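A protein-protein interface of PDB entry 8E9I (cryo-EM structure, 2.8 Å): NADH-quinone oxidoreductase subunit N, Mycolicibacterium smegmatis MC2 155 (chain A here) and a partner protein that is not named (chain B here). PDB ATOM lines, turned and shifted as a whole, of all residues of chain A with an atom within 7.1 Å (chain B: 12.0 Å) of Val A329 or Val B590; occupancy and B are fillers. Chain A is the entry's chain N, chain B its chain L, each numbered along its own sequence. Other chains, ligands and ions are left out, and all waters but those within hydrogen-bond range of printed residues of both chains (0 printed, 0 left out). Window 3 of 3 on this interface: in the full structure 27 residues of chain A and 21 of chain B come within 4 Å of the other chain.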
ATOM      1  N   VAL A 323     -16.811   2.412  -7.835  1.00  0.00           N
ATOM      2  CA  VAL A 323     -16.042   3.494  -8.434  1.00  0.00           C
ATOM      3  C   VAL A 323     -16.732   4.006  -9.682  1.00  0.00           C
ATOM      4  O   VAL A 323     -16.757   5.216  -9.937  1.00  0.00           O
ATOM      5  CB  VAL A 323     -14.612   3.019  -8.741  1.00  0.00           C
ATOM      6  CG1 VAL A 323     -13.884   4.033  -9.598  1.00  0.00           C
ATOM      7  CG2 VAL A 323     -13.848   2.762  -7.458  1.00  0.00           C
ATOM      8  N   GLY A 324     -17.299   3.108 -10.482  1.00  0.00           N
ATOM      9  CA  GLY A 324     -18.016   3.545 -11.666  1.00  0.00           C
ATOM     10  C   GLY A 324     -19.171   4.464 -11.329  1.00  0.00           C
ATOM     11  O   GLY A 324     -19.404   5.465 -12.010  1.00  0.00           O
ATOM     12  N   THR A 325     -19.910   4.142 -10.268  1.00  0.00           N
ATOM     13  CA  THR A 325     -21.089   4.936  -9.945  1.00  0.00           C
ATOM     14  C   THR A 325     -20.713   6.165  -9.132  1.00  0.00           C
ATOM     15  O   THR A 325     -21.153   7.279  -9.436  1.00  0.00           O
ATOM     16  CB  THR A 325     -22.115   4.089  -9.195  1.00  0.00           C
ATOM     17  OG1 THR A 325     -21.487   3.439  -8.085  1.00  0.00           O
ATOM     18  CG2 THR A 325     -22.732   3.052 -10.117  1.00  0.00           C
ATOM     19  N   VAL A 326     -19.890   5.989  -8.099  1.00  0.00           N
ATOM     20  CA  VAL A 326     -19.556   7.117  -7.237  1.00  0.00           C
ATOM     21  C   VAL A 326     -18.865   8.208  -8.043  1.00  0.00           C
ATOM     22  O   VAL A 326     -19.209   9.391  -7.937  1.00  0.00           O
ATOM     23  CB  VAL A 326     -18.693   6.648  -6.053  1.00  0.00           C
ATOM     24  CG1 VAL A 326     -18.292   7.826  -5.195  1.00  0.00           C
ATOM     25  CG2 VAL A 326     -19.444   5.627  -5.220  1.00  0.00           C
ATOM     26  N   THR A 327     -17.905   7.830  -8.885  1.00  0.00           N
ATOM     27  CA  THR A 327     -17.223   8.814  -9.715  1.00  0.00           C
ATOM     28  C   THR A 327     -18.196   9.570 -10.610  1.00  0.00           C
ATOM     29  O   THR A 327     -17.913  10.704 -11.008  1.00  0.00           O
ATOM     30  CB  THR A 327     -16.158   8.127 -10.564  1.00  0.00           C
ATOM     31  OG1 THR A 327     -15.350   7.290  -9.729  1.00  0.00           O
ATOM     32  CG2 THR A 327     -15.281   9.146 -11.257  1.00  0.00           C
ATOM     33  N   ALA A 328     -19.334   8.959 -10.946  1.00  0.00           N
ATOM     34  CA  ALA A 328     -20.310   9.628 -11.797  1.00  0.00           C
ATOM     35  C   ALA A 328     -21.166  10.612 -11.016  1.00  0.00           C
ATOM     36  O   ALA A 328     -21.721  11.546 -11.603  1.00  0.00           O
ATOM     37  CB  ALA A 328     -21.208   8.600 -12.477  1.00  0.00           C
ATOM     38  N   VAL A 329     -21.283  10.422  -9.701  1.00  0.00           N
ATOM     39  CA  VAL A 329     -22.199  11.236  -8.905  1.00  0.00           C
ATOM     40  C   VAL A 329     -21.894  12.714  -9.092  1.00  0.00           C
ATOM     41  O   VAL A 329     -22.799  13.539  -9.263  1.00  0.00           O
ATOM     42  CB  VAL A 329     -22.115  10.834  -7.422  1.00  0.00           C
ATOM     43  CG1 VAL A 329     -22.712  11.917  -6.542  1.00  0.00           C
ATOM     44  CG2 VAL A 329     -22.820   9.510  -7.199  1.00  0.00           C
ATOM     45  N   THR A 330     -20.613  13.068  -9.056  1.00  0.00           N
ATOM     46  CA  THR A 330     -20.203  14.459  -9.161  1.00  0.00           C
ATOM     47  C   THR A 330     -19.593  14.801 -10.511  1.00  0.00           C
ATOM     48  O   THR A 330     -18.819  15.759 -10.594  1.00  0.00           O
ATOM     49  CB  THR A 330     -19.211  14.790  -8.047  1.00  0.00           C
ATOM     50  OG1 THR A 330     -19.132  16.211  -7.886  1.00  0.00           O
ATOM     51  CG2 THR A 330     -17.838  14.235  -8.371  1.00  0.00           C
ATOM     52  N   GLN A 331     -19.894  14.041 -11.557  1.00  0.00           N
ATOM     53  CA  GLN A 331     -19.459  14.417 -12.893  1.00  0.00           C
ATOM     54  C   GLN A 331     -20.411  15.458 -13.469  1.00  0.00           C
ATOM     55  O   GLN A 331     -21.631  15.355 -13.316  1.00  0.00           O
ATOM     56  CB  GLN A 331     -19.404  13.185 -13.795  1.00  0.00           C
ATOM     57  CG  GLN A 331     -18.571  13.358 -15.046  1.00  0.00           C
ATOM     58  CD  GLN A 331     -17.178  13.859 -14.754  1.00  0.00           C
ATOM     59  OE1 GLN A 331     -16.854  15.014 -15.021  1.00  0.00           O
ATOM     60  NE2 GLN A 331     -16.341  12.990 -14.206  1.00  0.00           N
ATOM     61  N   THR A 332     -19.850  16.463 -14.141  1.00  0.00           N
ATOM     62  CA  THR A 332     -20.614  17.623 -14.579  1.00  0.00           C
ATOM     63  C   THR A 332     -20.830  17.696 -16.083  1.00  0.00           C
ATOM     64  O   THR A 332     -21.460  18.650 -16.551  1.00  0.00           O
ATOM     65  CB  THR A 332     -19.915  18.910 -14.131  1.00  0.00           C
ATOM     66  OG1 THR A 332     -18.624  18.985 -14.746  1.00  0.00           O
ATOM     67  CG2 THR A 332     -19.757  18.929 -12.624  1.00  0.00           C
ATOM     68  N   MET A 337     -20.585  11.728 -17.961  1.00  0.00           N
ATOM     69  CA  MET A 337     -21.479  11.029 -17.046  1.00  0.00           C
ATOM     70  C   MET A 337     -21.993   9.735 -17.661  1.00  0.00           C
ATOM     71  O   MET A 337     -22.050   8.700 -16.992  1.00  0.00           O
ATOM     72  CB  MET A 337     -22.640  11.941 -16.660  1.00  0.00           C
ATOM     73  CG  MET A 337     -23.598  11.334 -15.662  1.00  0.00           C
ATOM     74  SD  MET A 337     -24.794  10.245 -16.445  1.00  0.00           S
ATOM     75  CE  MET A 337     -25.826  11.437 -17.276  1.00  0.00           C
ATOM     76  N   TYR A 340     -19.280   7.152 -17.462  1.00  0.00           N
ATOM     77  CA  TYR A 340     -19.196   6.473 -16.174  1.00  0.00           C
ATOM     78  C   TYR A 340     -20.393   5.565 -15.941  1.00  0.00           C
ATOM     79  O   TYR A 340     -20.274   4.540 -15.259  1.00  0.00           O
ATOM     80  CB  TYR A 340     -19.074   7.483 -15.044  1.00  0.00           C
ATOM     81  CG  TYR A 340     -17.702   8.073 -14.941  1.00  0.00           C
ATOM     82  CD1 TYR A 340     -16.657   7.339 -14.416  1.00  0.00           C
ATOM     83  CD2 TYR A 340     -17.448   9.358 -15.376  1.00  0.00           C
ATOM     84  CE1 TYR A 340     -15.399   7.869 -14.322  1.00  0.00           C
ATOM     85  CE2 TYR A 340     -16.193   9.898 -15.285  1.00  0.00           C
ATOM     86  CZ  TYR A 340     -15.173   9.149 -14.758  1.00  0.00           C
ATOM     87  OH  TYR A 340     -13.921   9.687 -14.667  1.00  0.00           O
ATOM     88  N   MET A 396     -23.683  20.014 -18.233  1.00  0.00           N
ATOM     89  CA  MET A 396     -25.032  19.819 -17.720  1.00  0.00           C
ATOM     90  C   MET A 396     -25.758  21.140 -17.514  1.00  0.00           C
ATOM     91  O   MET A 396     -26.981  21.202 -17.675  1.00  0.00           O
ATOM     92  CB  MET A 396     -24.980  19.026 -16.416  1.00  0.00           C
ATOM     93  CG  MET A 396     -24.509  17.596 -16.587  1.00  0.00           C
ATOM     94  SD  MET A 396     -24.381  16.739 -15.015  1.00  0.00           S
ATOM     95  CE  MET A 396     -26.108  16.572 -14.590  1.00  0.00           C
ATOM     96  N   VAL A 457     -27.045   4.686  -5.566  1.00  0.00           N
ATOM     97  CA  VAL A 457     -26.165   5.846  -5.679  1.00  0.00           C
ATOM     98  C   VAL A 457     -26.247   6.446  -7.078  1.00  0.00           C
ATOM     99  O   VAL A 457     -26.207   7.669  -7.248  1.00  0.00           O
ATOM    100  CB  VAL A 457     -24.723   5.460  -5.313  1.00  0.00           C
ATOM    101  CG1 VAL A 457     -23.753   6.540  -5.761  1.00  0.00           C
ATOM    102  CG2 VAL A 457     -24.609   5.224  -3.822  1.00  0.00           C
ATOM    103  N   ALA A 458     -26.356   5.595  -8.100  1.00  0.00           N
ATOM    104  CA  ALA A 458     -26.316   6.077  -9.478  1.00  0.00           C
ATOM    105  C   ALA A 458     -27.619   6.758  -9.873  1.00  0.00           C
ATOM    106  O   ALA A 458     -27.631   7.634 -10.752  1.00  0.00           O
ATOM    107  CB  ALA A 458     -26.017   4.918 -10.424  1.00  0.00           C
ATOM    108  N   ALA A 459     -28.727   6.352  -9.256  1.00  0.00           N
ATOM    109  CA  ALA A 459     -30.000   6.986  -9.558  1.00  0.00           C
ATOM    110  C   ALA A 459     -29.910   8.487  -9.354  1.00  0.00           C
ATOM    111  O   ALA A 459     -30.585   9.254 -10.043  1.00  0.00           O
ATOM    112  CB  ALA A 459     -31.102   6.393  -8.684  1.00  0.00           C
ATOM    113  N   TYR A 460     -29.063   8.928  -8.425  1.00  0.00           N
ATOM    114  CA  TYR A 460     -28.936  10.356  -8.166  1.00  0.00           C
ATOM    115  C   TYR A 460     -28.450  11.103  -9.399  1.00  0.00           C
ATOM    116  O   TYR A 460     -29.036  12.117  -9.795  1.00  0.00           O
ATOM    117  CB  TYR A 460     -27.986  10.601  -7.000  1.00  0.00           C
ATOM    118  CG  TYR A 460     -27.554  12.038  -6.897  1.00  0.00           C
ATOM    119  CD1 TYR A 460     -28.339  12.969  -6.243  1.00  0.00           C
ATOM    120  CD2 TYR A 460     -26.371  12.469  -7.470  1.00  0.00           C
ATOM    121  CE1 TYR A 460     -27.955  14.283  -6.147  1.00  0.00           C
ATOM    122  CE2 TYR A 460     -25.978  13.786  -7.382  1.00  0.00           C
ATOM    123  CZ  TYR A 460     -26.776  14.689  -6.721  1.00  0.00           C
ATOM    124  OH  TYR A 460     -26.389  16.003  -6.627  1.00  0.00           O
ATOM    125  N   PHE A 461     -27.359  10.638 -10.007  1.00  0.00           N
ATOM    126  CA  PHE A 461     -26.840  11.354 -11.163  1.00  0.00           C
ATOM    127  C   PHE A 461     -27.678  11.095 -12.402  1.00  0.00           C
ATOM    128  O   PHE A 461     -27.664  11.909 -13.330  1.00  0.00           O
ATOM    129  CB  PHE A 461     -25.370  11.001 -11.409  1.00  0.00           C
ATOM    130  CG  PHE A 461     -25.143   9.647 -12.014  1.00  0.00           C
ATOM    131  CD1 PHE A 461     -25.399   9.412 -13.349  1.00  0.00           C
ATOM    132  CD2 PHE A 461     -24.617   8.623 -11.258  1.00  0.00           C
ATOM    133  CE1 PHE A 461     -25.173   8.173 -13.903  1.00  0.00           C
ATOM    134  CE2 PHE A 461     -24.385   7.385 -11.807  1.00  0.00           C
ATOM    135  CZ  PHE A 461     -24.662   7.160 -13.129  1.00  0.00           C
ATOM    136  N   ARG A 464     -30.556  13.802 -11.606  1.00  0.00           N
ATOM    137  CA  ARG A 464     -30.196  15.210 -11.689  1.00  0.00           C
ATOM    138  C   ARG A 464     -30.318  15.724 -13.114  1.00  0.00           C
ATOM    139  O   ARG A 464     -30.657  16.891 -13.333  1.00  0.00           O
ATOM    140  CB  ARG A 464     -28.776  15.424 -11.163  1.00  0.00           C
ATOM    141  N   GLY B 581     -29.743  15.146   9.166  1.00  0.00           N
ATOM    142  CA  GLY B 581     -28.298  15.230   9.183  1.00  0.00           C
ATOM    143  C   GLY B 581     -27.606  13.940   8.817  1.00  0.00           C
ATOM    144  O   GLY B 581     -26.555  13.981   8.180  1.00  0.00           O
ATOM    145  N   THR B 582     -28.167  12.795   9.203  1.00  0.00           N
ATOM    146  CA  THR B 582     -27.560  11.529   8.808  1.00  0.00           C
ATOM    147  C   THR B 582     -27.605  11.344   7.296  1.00  0.00           C
ATOM    148  O   THR B 582     -26.597  10.978   6.677  1.00  0.00           O
ATOM    149  CB  THR B 582     -28.267  10.366   9.501  1.00  0.00           C
ATOM    150  OG1 THR B 582     -29.684  10.550   9.420  1.00  0.00           O
ATOM    151  CG2 THR B 582     -27.860  10.290  10.965  1.00  0.00           C
ATOM    152  N   ALA B 583     -28.761  11.602   6.682  1.00  0.00           N
ATOM    153  CA  ALA B 583     -28.858  11.496   5.232  1.00  0.00           C
ATOM    154  C   ALA B 583     -27.941  12.499   4.551  1.00  0.00           C
ATOM    155  O   ALA B 583     -27.285  12.174   3.556  1.00  0.00           O
ATOM    156  CB  ALA B 583     -30.303  11.705   4.785  1.00  0.00           C
ATOM    157  N   GLY B 584     -27.882  13.723   5.071  1.00  0.00           N
ATOM    158  CA  GLY B 584     -26.997  14.716   4.488  1.00  0.00           C
ATOM    159  C   GLY B 584     -25.537  14.331   4.611  1.00  0.00           C
ATOM    160  O   GLY B 584     -24.741  14.590   3.711  1.00  0.00           O
ATOM    161  N   GLY B 585     -25.166  13.714   5.731  1.00  0.00           N
ATOM    162  CA  GLY B 585     -23.799  13.253   5.892  1.00  0.00           C
ATOM    163  C   GLY B 585     -23.465  12.124   4.943  1.00  0.00           C
ATOM    164  O   GLY B 585     -22.359  12.057   4.410  1.00  0.00           O
ATOM    165  N   LEU B 586     -24.417  11.217   4.721  1.00  0.00           N
ATOM    166  CA  LEU B 586     -24.201  10.177   3.721  1.00  0.00           C
ATOM    167  C   LEU B 586     -24.048  10.784   2.334  1.00  0.00           C
ATOM    168  O   LEU B 586     -23.195  10.353   1.549  1.00  0.00           O
ATOM    169  CB  LEU B 586     -25.347   9.171   3.751  1.00  0.00           C
ATOM    170  CG  LEU B 586     -25.150   7.977   2.817  1.00  0.00           C
ATOM    171  CD1 LEU B 586     -25.634   6.701   3.469  1.00  0.00           C
ATOM    172  CD2 LEU B 586     -25.880   8.199   1.507  1.00  0.00           C
ATOM    173  N   ALA B 587     -24.855  11.797   2.020  1.00  0.00           N
ATOM    174  CA  ALA B 587     -24.712  12.477   0.738  1.00  0.00           C
ATOM    175  C   ALA B 587     -23.351  13.153   0.623  1.00  0.00           C
ATOM    176  O   ALA B 587     -22.707  13.092  -0.428  1.00  0.00           O
ATOM    177  CB  ALA B 587     -25.835  13.499   0.560  1.00  0.00           C
ATOM    178  N   ALA B 588     -22.904  13.814   1.690  1.00  0.00           N
ATOM    179  CA  ALA B 588     -21.611  14.486   1.661  1.00  0.00           C
ATOM    180  C   ALA B 588     -20.480  13.481   1.522  1.00  0.00           C
ATOM    181  O   ALA B 588     -19.490  13.748   0.838  1.00  0.00           O
ATOM    182  CB  ALA B 588     -21.425  15.328   2.923  1.00  0.00           C
ATOM    183  N   LEU B 589     -20.606  12.328   2.175  1.00  0.00           N
ATOM    184  CA  LEU B 589     -19.623  11.267   2.007  1.00  0.00           C
ATOM    185  C   LEU B 589     -19.577  10.800   0.560  1.00  0.00           C
ATOM    186  O   LEU B 589     -18.501  10.659  -0.027  1.00  0.00           O
ATOM    187  CB  LEU B 589     -19.954  10.105   2.940  1.00  0.00           C
ATOM    188  CG  LEU B 589     -19.220   8.791   2.674  1.00  0.00           C
ATOM    189  CD1 LEU B 589     -17.733   8.957   2.924  1.00  0.00           C
ATOM    190  CD2 LEU B 589     -19.790   7.688   3.539  1.00  0.00           C
ATOM    191  N   VAL B 590     -20.745  10.560  -0.035  1.00  0.00           N
ATOM    192  CA  VAL B 590     -20.781  10.129  -1.428  1.00  0.00           C
ATOM    193  C   VAL B 590     -20.143  11.179  -2.323  1.00  0.00           C
ATOM    194  O   VAL B 590     -19.370  10.855  -3.229  1.00  0.00           O
ATOM    195  CB  VAL B 590     -22.225   9.823  -1.860  1.00  0.00           C
ATOM    196  CG1 VAL B 590     -22.304   9.668  -3.367  1.00  0.00           C
ATOM    197  CG2 VAL B 590     -22.718   8.563  -1.176  1.00  0.00           C
ATOM    198  N   SER B 591     -20.445  12.453  -2.082  1.00  0.00           N
ATOM    199  CA  SER B 591     -19.936  13.513  -2.946  1.00  0.00           C
ATOM    200  C   SER B 591     -18.428  13.677  -2.791  1.00  0.00           C
ATOM    201  O   SER B 591     -17.703  13.851  -3.778  1.00  0.00           O
ATOM    202  CB  SER B 591     -20.653  14.824  -2.632  1.00  0.00           C
ATOM    203  OG  SER B 591     -22.053  14.675  -2.766  1.00  0.00           O
ATOM    204  N   ARG B 592     -17.935  13.637  -1.555  1.00  0.00           N
ATOM    205  CA  ARG B 592     -16.500  13.732  -1.327  1.00  0.00           C
ATOM    206  C   ARG B 592     -15.770  12.554  -1.952  1.00  0.00           C
ATOM    207  O   ARG B 592     -14.708  12.719  -2.562  1.00  0.00           O
ATOM    208  CB  ARG B 592     -16.218  13.807   0.170  1.00  0.00           C
ATOM    209  CG  ARG B 592     -16.466  15.169   0.781  1.00  0.00           C
ATOM    210  CD  ARG B 592     -16.250  15.126   2.284  1.00  0.00           C
ATOM    211  NE  ARG B 592     -14.939  14.581   2.618  1.00  0.00           N
ATOM    212  CZ  ARG B 592     -14.732  13.461   3.303  1.00  0.00           C
ATOM    213  NH1 ARG B 592     -15.734  12.738   3.780  1.00  0.00           N
ATOM    214  NH2 ARG B 592     -13.483  13.053   3.512  1.00  0.00           N
ATOM    215  N   THR B 593     -16.321  11.348  -1.805  1.00  0.00           N
ATOM    216  CA  THR B 593     -15.695  10.186  -2.419  1.00  0.00           C
ATOM    217  C   THR B 593     -15.723  10.296  -3.932  1.00  0.00           C
ATOM    218  O   THR B 593     -14.779   9.882  -4.608  1.00  0.00           O
ATOM    219  CB  THR B 593     -16.395   8.909  -1.968  1.00  0.00           C
ATOM    220  OG1 THR B 593     -16.457   8.874  -0.540  1.00  0.00           O
ATOM    221  CG2 THR B 593     -15.642   7.695  -2.464  1.00  0.00           C
ATOM    222  N   SER B 594     -16.801  10.847  -4.485  1.00  0.00           N
ATOM    223  CA  SER B 594     -16.870  11.046  -5.925  1.00  0.00           C
ATOM    224  C   SER B 594     -15.793  12.012  -6.386  1.00  0.00           C
ATOM    225  O   SER B 594     -15.125  11.778  -7.395  1.00  0.00           O
ATOM    226  CB  SER B 594     -18.254  11.553  -6.318  1.00  0.00           C
ATOM    227  OG  SER B 594     -18.443  11.465  -7.717  1.00  0.00           O
ATOM    228  N   ASP B 595     -15.608  13.108  -5.659  1.00  0.00           N
ATOM    229  CA  ASP B 595     -14.547  14.041  -6.022  1.00  0.00           C
ATOM    230  C   ASP B 595     -13.179  13.375  -5.932  1.00  0.00           C
ATOM    231  O   ASP B 595     -12.345  13.525  -6.834  1.00  0.00           O
ATOM    232  CB  ASP B 595     -14.608  15.275  -5.124  1.00  0.00           C
ATOM    233  N   ALA B 596     -12.936  12.619  -4.861  1.00  0.00           N
ATOM    234  CA  ALA B 596     -11.641  11.974  -4.687  1.00  0.00           C
ATOM    235  C   ALA B 596     -11.373  10.976  -5.805  1.00  0.00           C
ATOM    236  O   ALA B 596     -10.261  10.906  -6.337  1.00  0.00           O
ATOM    237  CB  ALA B 596     -11.581  11.287  -3.324  1.00  0.00           C
ATOM    238  N   LEU B 597     -12.383  10.186  -6.169  1.00  0.00           N
ATOM    239  CA  LEU B 597     -12.227   9.249  -7.276  1.00  0.00           C
ATOM    240  C   LEU B 597     -11.998   9.983  -8.585  1.00  0.00           C
ATOM    241  O   LEU B 597     -11.130   9.603  -9.378  1.00  0.00           O
ATOM    242  CB  LEU B 597     -13.462   8.360  -7.381  1.00  0.00           C
ATOM    243  CG  LEU B 597     -13.582   7.263  -6.331  1.00  0.00           C
ATOM    244  CD1 LEU B 597     -14.998   6.750  -6.282  1.00  0.00           C
ATOM    245  CD2 LEU B 597     -12.621   6.142  -6.652  1.00  0.00           C
ATOM    246  N   ARG B 598     -12.766  11.044  -8.830  1.00  0.00           N
ATOM    247  CA  ARG B 598     -12.625  11.799 -10.065  1.00  0.00           C
ATOM    248  C   ARG B 598     -11.235  12.400 -10.192  1.00  0.00           C
ATOM    249  O   ARG B 598     -10.745  12.600 -11.307  1.00  0.00           O
ATOM    250  CB  ARG B 598     -13.695  12.883 -10.117  1.00  0.00           C
ATOM    251  CG  ARG B 598     -13.710  13.694 -11.386  1.00  0.00           C
ATOM    252  CD  ARG B 598     -15.008  14.466 -11.498  1.00  0.00           C
ATOM    253  NE  ARG B 598     -15.245  15.262 -10.302  1.00  0.00           N
ATOM    254  CZ  ARG B 598     -14.951  16.548 -10.177  1.00  0.00           C
ATOM    255  NH1 ARG B 598     -14.382  17.229 -11.159  1.00  0.00           N
ATOM    256  NH2 ARG B 598     -15.222  17.165  -9.032  1.00  0.00           N
ATOM    257  N   GLN B 599     -10.590  12.705  -9.066  1.00  0.00           N
ATOM    258  CA  GLN B 599      -9.191  13.111  -9.129  1.00  0.00           C
ATOM    259  C   GLN B 599      -8.307  12.005  -9.692  1.00  0.00           C
ATOM    260  O   GLN B 599      -7.201  12.284 -10.160  1.00  0.00           O
ATOM    261  CB  GLN B 599      -8.686  13.520  -7.747  1.00  0.00           C
ATOM    262  CG  GLN B 599      -9.379  14.724  -7.142  1.00  0.00           C
ATOM    263  CD  GLN B 599      -9.563  15.855  -8.132  1.00  0.00           C
ATOM    264  OE1 GLN B 599      -8.595  16.353  -8.707  1.00  0.00           O
ATOM    265  NE2 GLN B 599     -10.809  16.270  -8.335  1.00  0.00           N
ATOM    266  N   GLN B 601      -8.779  10.334 -12.336  1.00  0.00           N
ATOM    267  CA  GLN B 601      -8.692  10.564 -13.777  1.00  0.00           C
ATOM    268  C   GLN B 601      -7.849  11.810 -14.057  1.00  0.00           C
ATOM    269  O   GLN B 601      -8.340  12.876 -14.423  1.00  0.00           O
ATOM    270  CB  GLN B 601     -10.082  10.692 -14.377  1.00  0.00           C
ATOM    271  CG  GLN B 601     -10.818   9.384 -14.468  1.00  0.00           C
ATOM    272  CD  GLN B 601     -10.406   8.559 -15.666  1.00  0.00           C
ATOM    273  OE1 GLN B 601      -9.818   7.490 -15.525  1.00  0.00           O
ATOM    274  NE2 GLN B 601     -10.719   9.052 -16.859  1.00  0.00           N
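The side-chain hydroxyl (OG) of Ser B594 is in hydrogen-bond range of the backbone carbonyl oxygen (O) of Thr A327 (3.4 Å).
O of Val A326 lies close to OG of Ser B594 (2.2 Å).
N of Thr A330 sits close to OG of Ser B594, at 3.0 Å.
O of Val A323 lies within hydrogen-bond range of OG1 of Thr A327, at 2.5 Å.
OG1 of Thr B593 is in hydrogen-bond range of O of Leu B589, at 2.8 Å.
O of Asp B595 lies close to NE2 of Gln B599 (3.5 Å).
CG2 of Val A323 touches CD2 of Leu B597, at 3.7 Å.
Val B590 touches Val A326.
CG1 of Val A326 touches C of Thr B593, at 3.8 Å.
Leu B597 touches Val A326 (CD1 to CG1, 3.6 Å).
OG1 of Thr A327 touches CB of Leu B597 (3.2 Å).
CA of Arg B598 touches CG2 of Thr A327, 3.9 Å away.
Val A329 touches Val B590 (CG2 to CG1, 3.9 Å).
N of Val A329 touches OG of Ser B594, 3.6 Å away.
Thr A330 touches Asp B595.
Thr A330 touches Arg B598 (CG2 to NE, 3.4 Å).
Printed residues of chain B within 4 Å of Val A323: Leu B597.
Gly A324 touches none of the printed residues of chain B.
No residue of chain B comes within 4 Å of Thr A325.
Val A326 touches four residues of chain B.
Of chain B, only Ser B594 (3.4 Å), Leu B597 (3.2 Å) and Arg B598 (3.9 Å) come within 4 Å of Thr A327.
No residue of chain B comes within 4 Å of Ala A328.
Val A329 touches just these residues of chain B: Val B590 and Ser B594.
Of chain B, only Ser B594, Asp B595 and Arg B598 come within 4 Å of Thr A330.
No residue of chain B comes within 4 Å of Val A457.
No residue of chain B comes within 4 Å of Tyr A460.
No residue of chain B comes within 4 Å of Phe A461.
Ala B588 touches none of the printed residues of chain A.
Of chain A, only Val A326 and Val A329 come within 4 Å of Val B590.
Of the printed residues of chain A, Thr B593 touches Val A326 (3.8 Å).
Of the printed residues of chain A, Asp B595 touches Thr A330 (3.7 Å).
Of the printed residues of chain A, Gln B601 touches Tyr A340 (3.1 Å).
The nearest residue of chain B that does not touch Val A329 is Ser B591 (4.7 Å).
Of the 20 printed residues of chain B, 7 touch a printed residue of chain A.
Printed residues of chain B that touch a printed residue of chain A: Val B590, Thr B593, Ser B594, Asp B595, Leu B597, Arg B598 and Gln B601.
Printed residues of chain A that touch a printed residue of chain B: Val A323, Val A326, Thr A327, Val A329, Thr A330, Gln A331 and Tyr A340.
Hydrophobic or aromatic side chains of chain A that line the printed part of chain B: Val A323, Val A326, Val A329 and Tyr A340.
Among the printed residues, no Asp or Glu carboxylate lies within 4 Å of a Lys or Arg side-chain nitrogen of the other chain.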
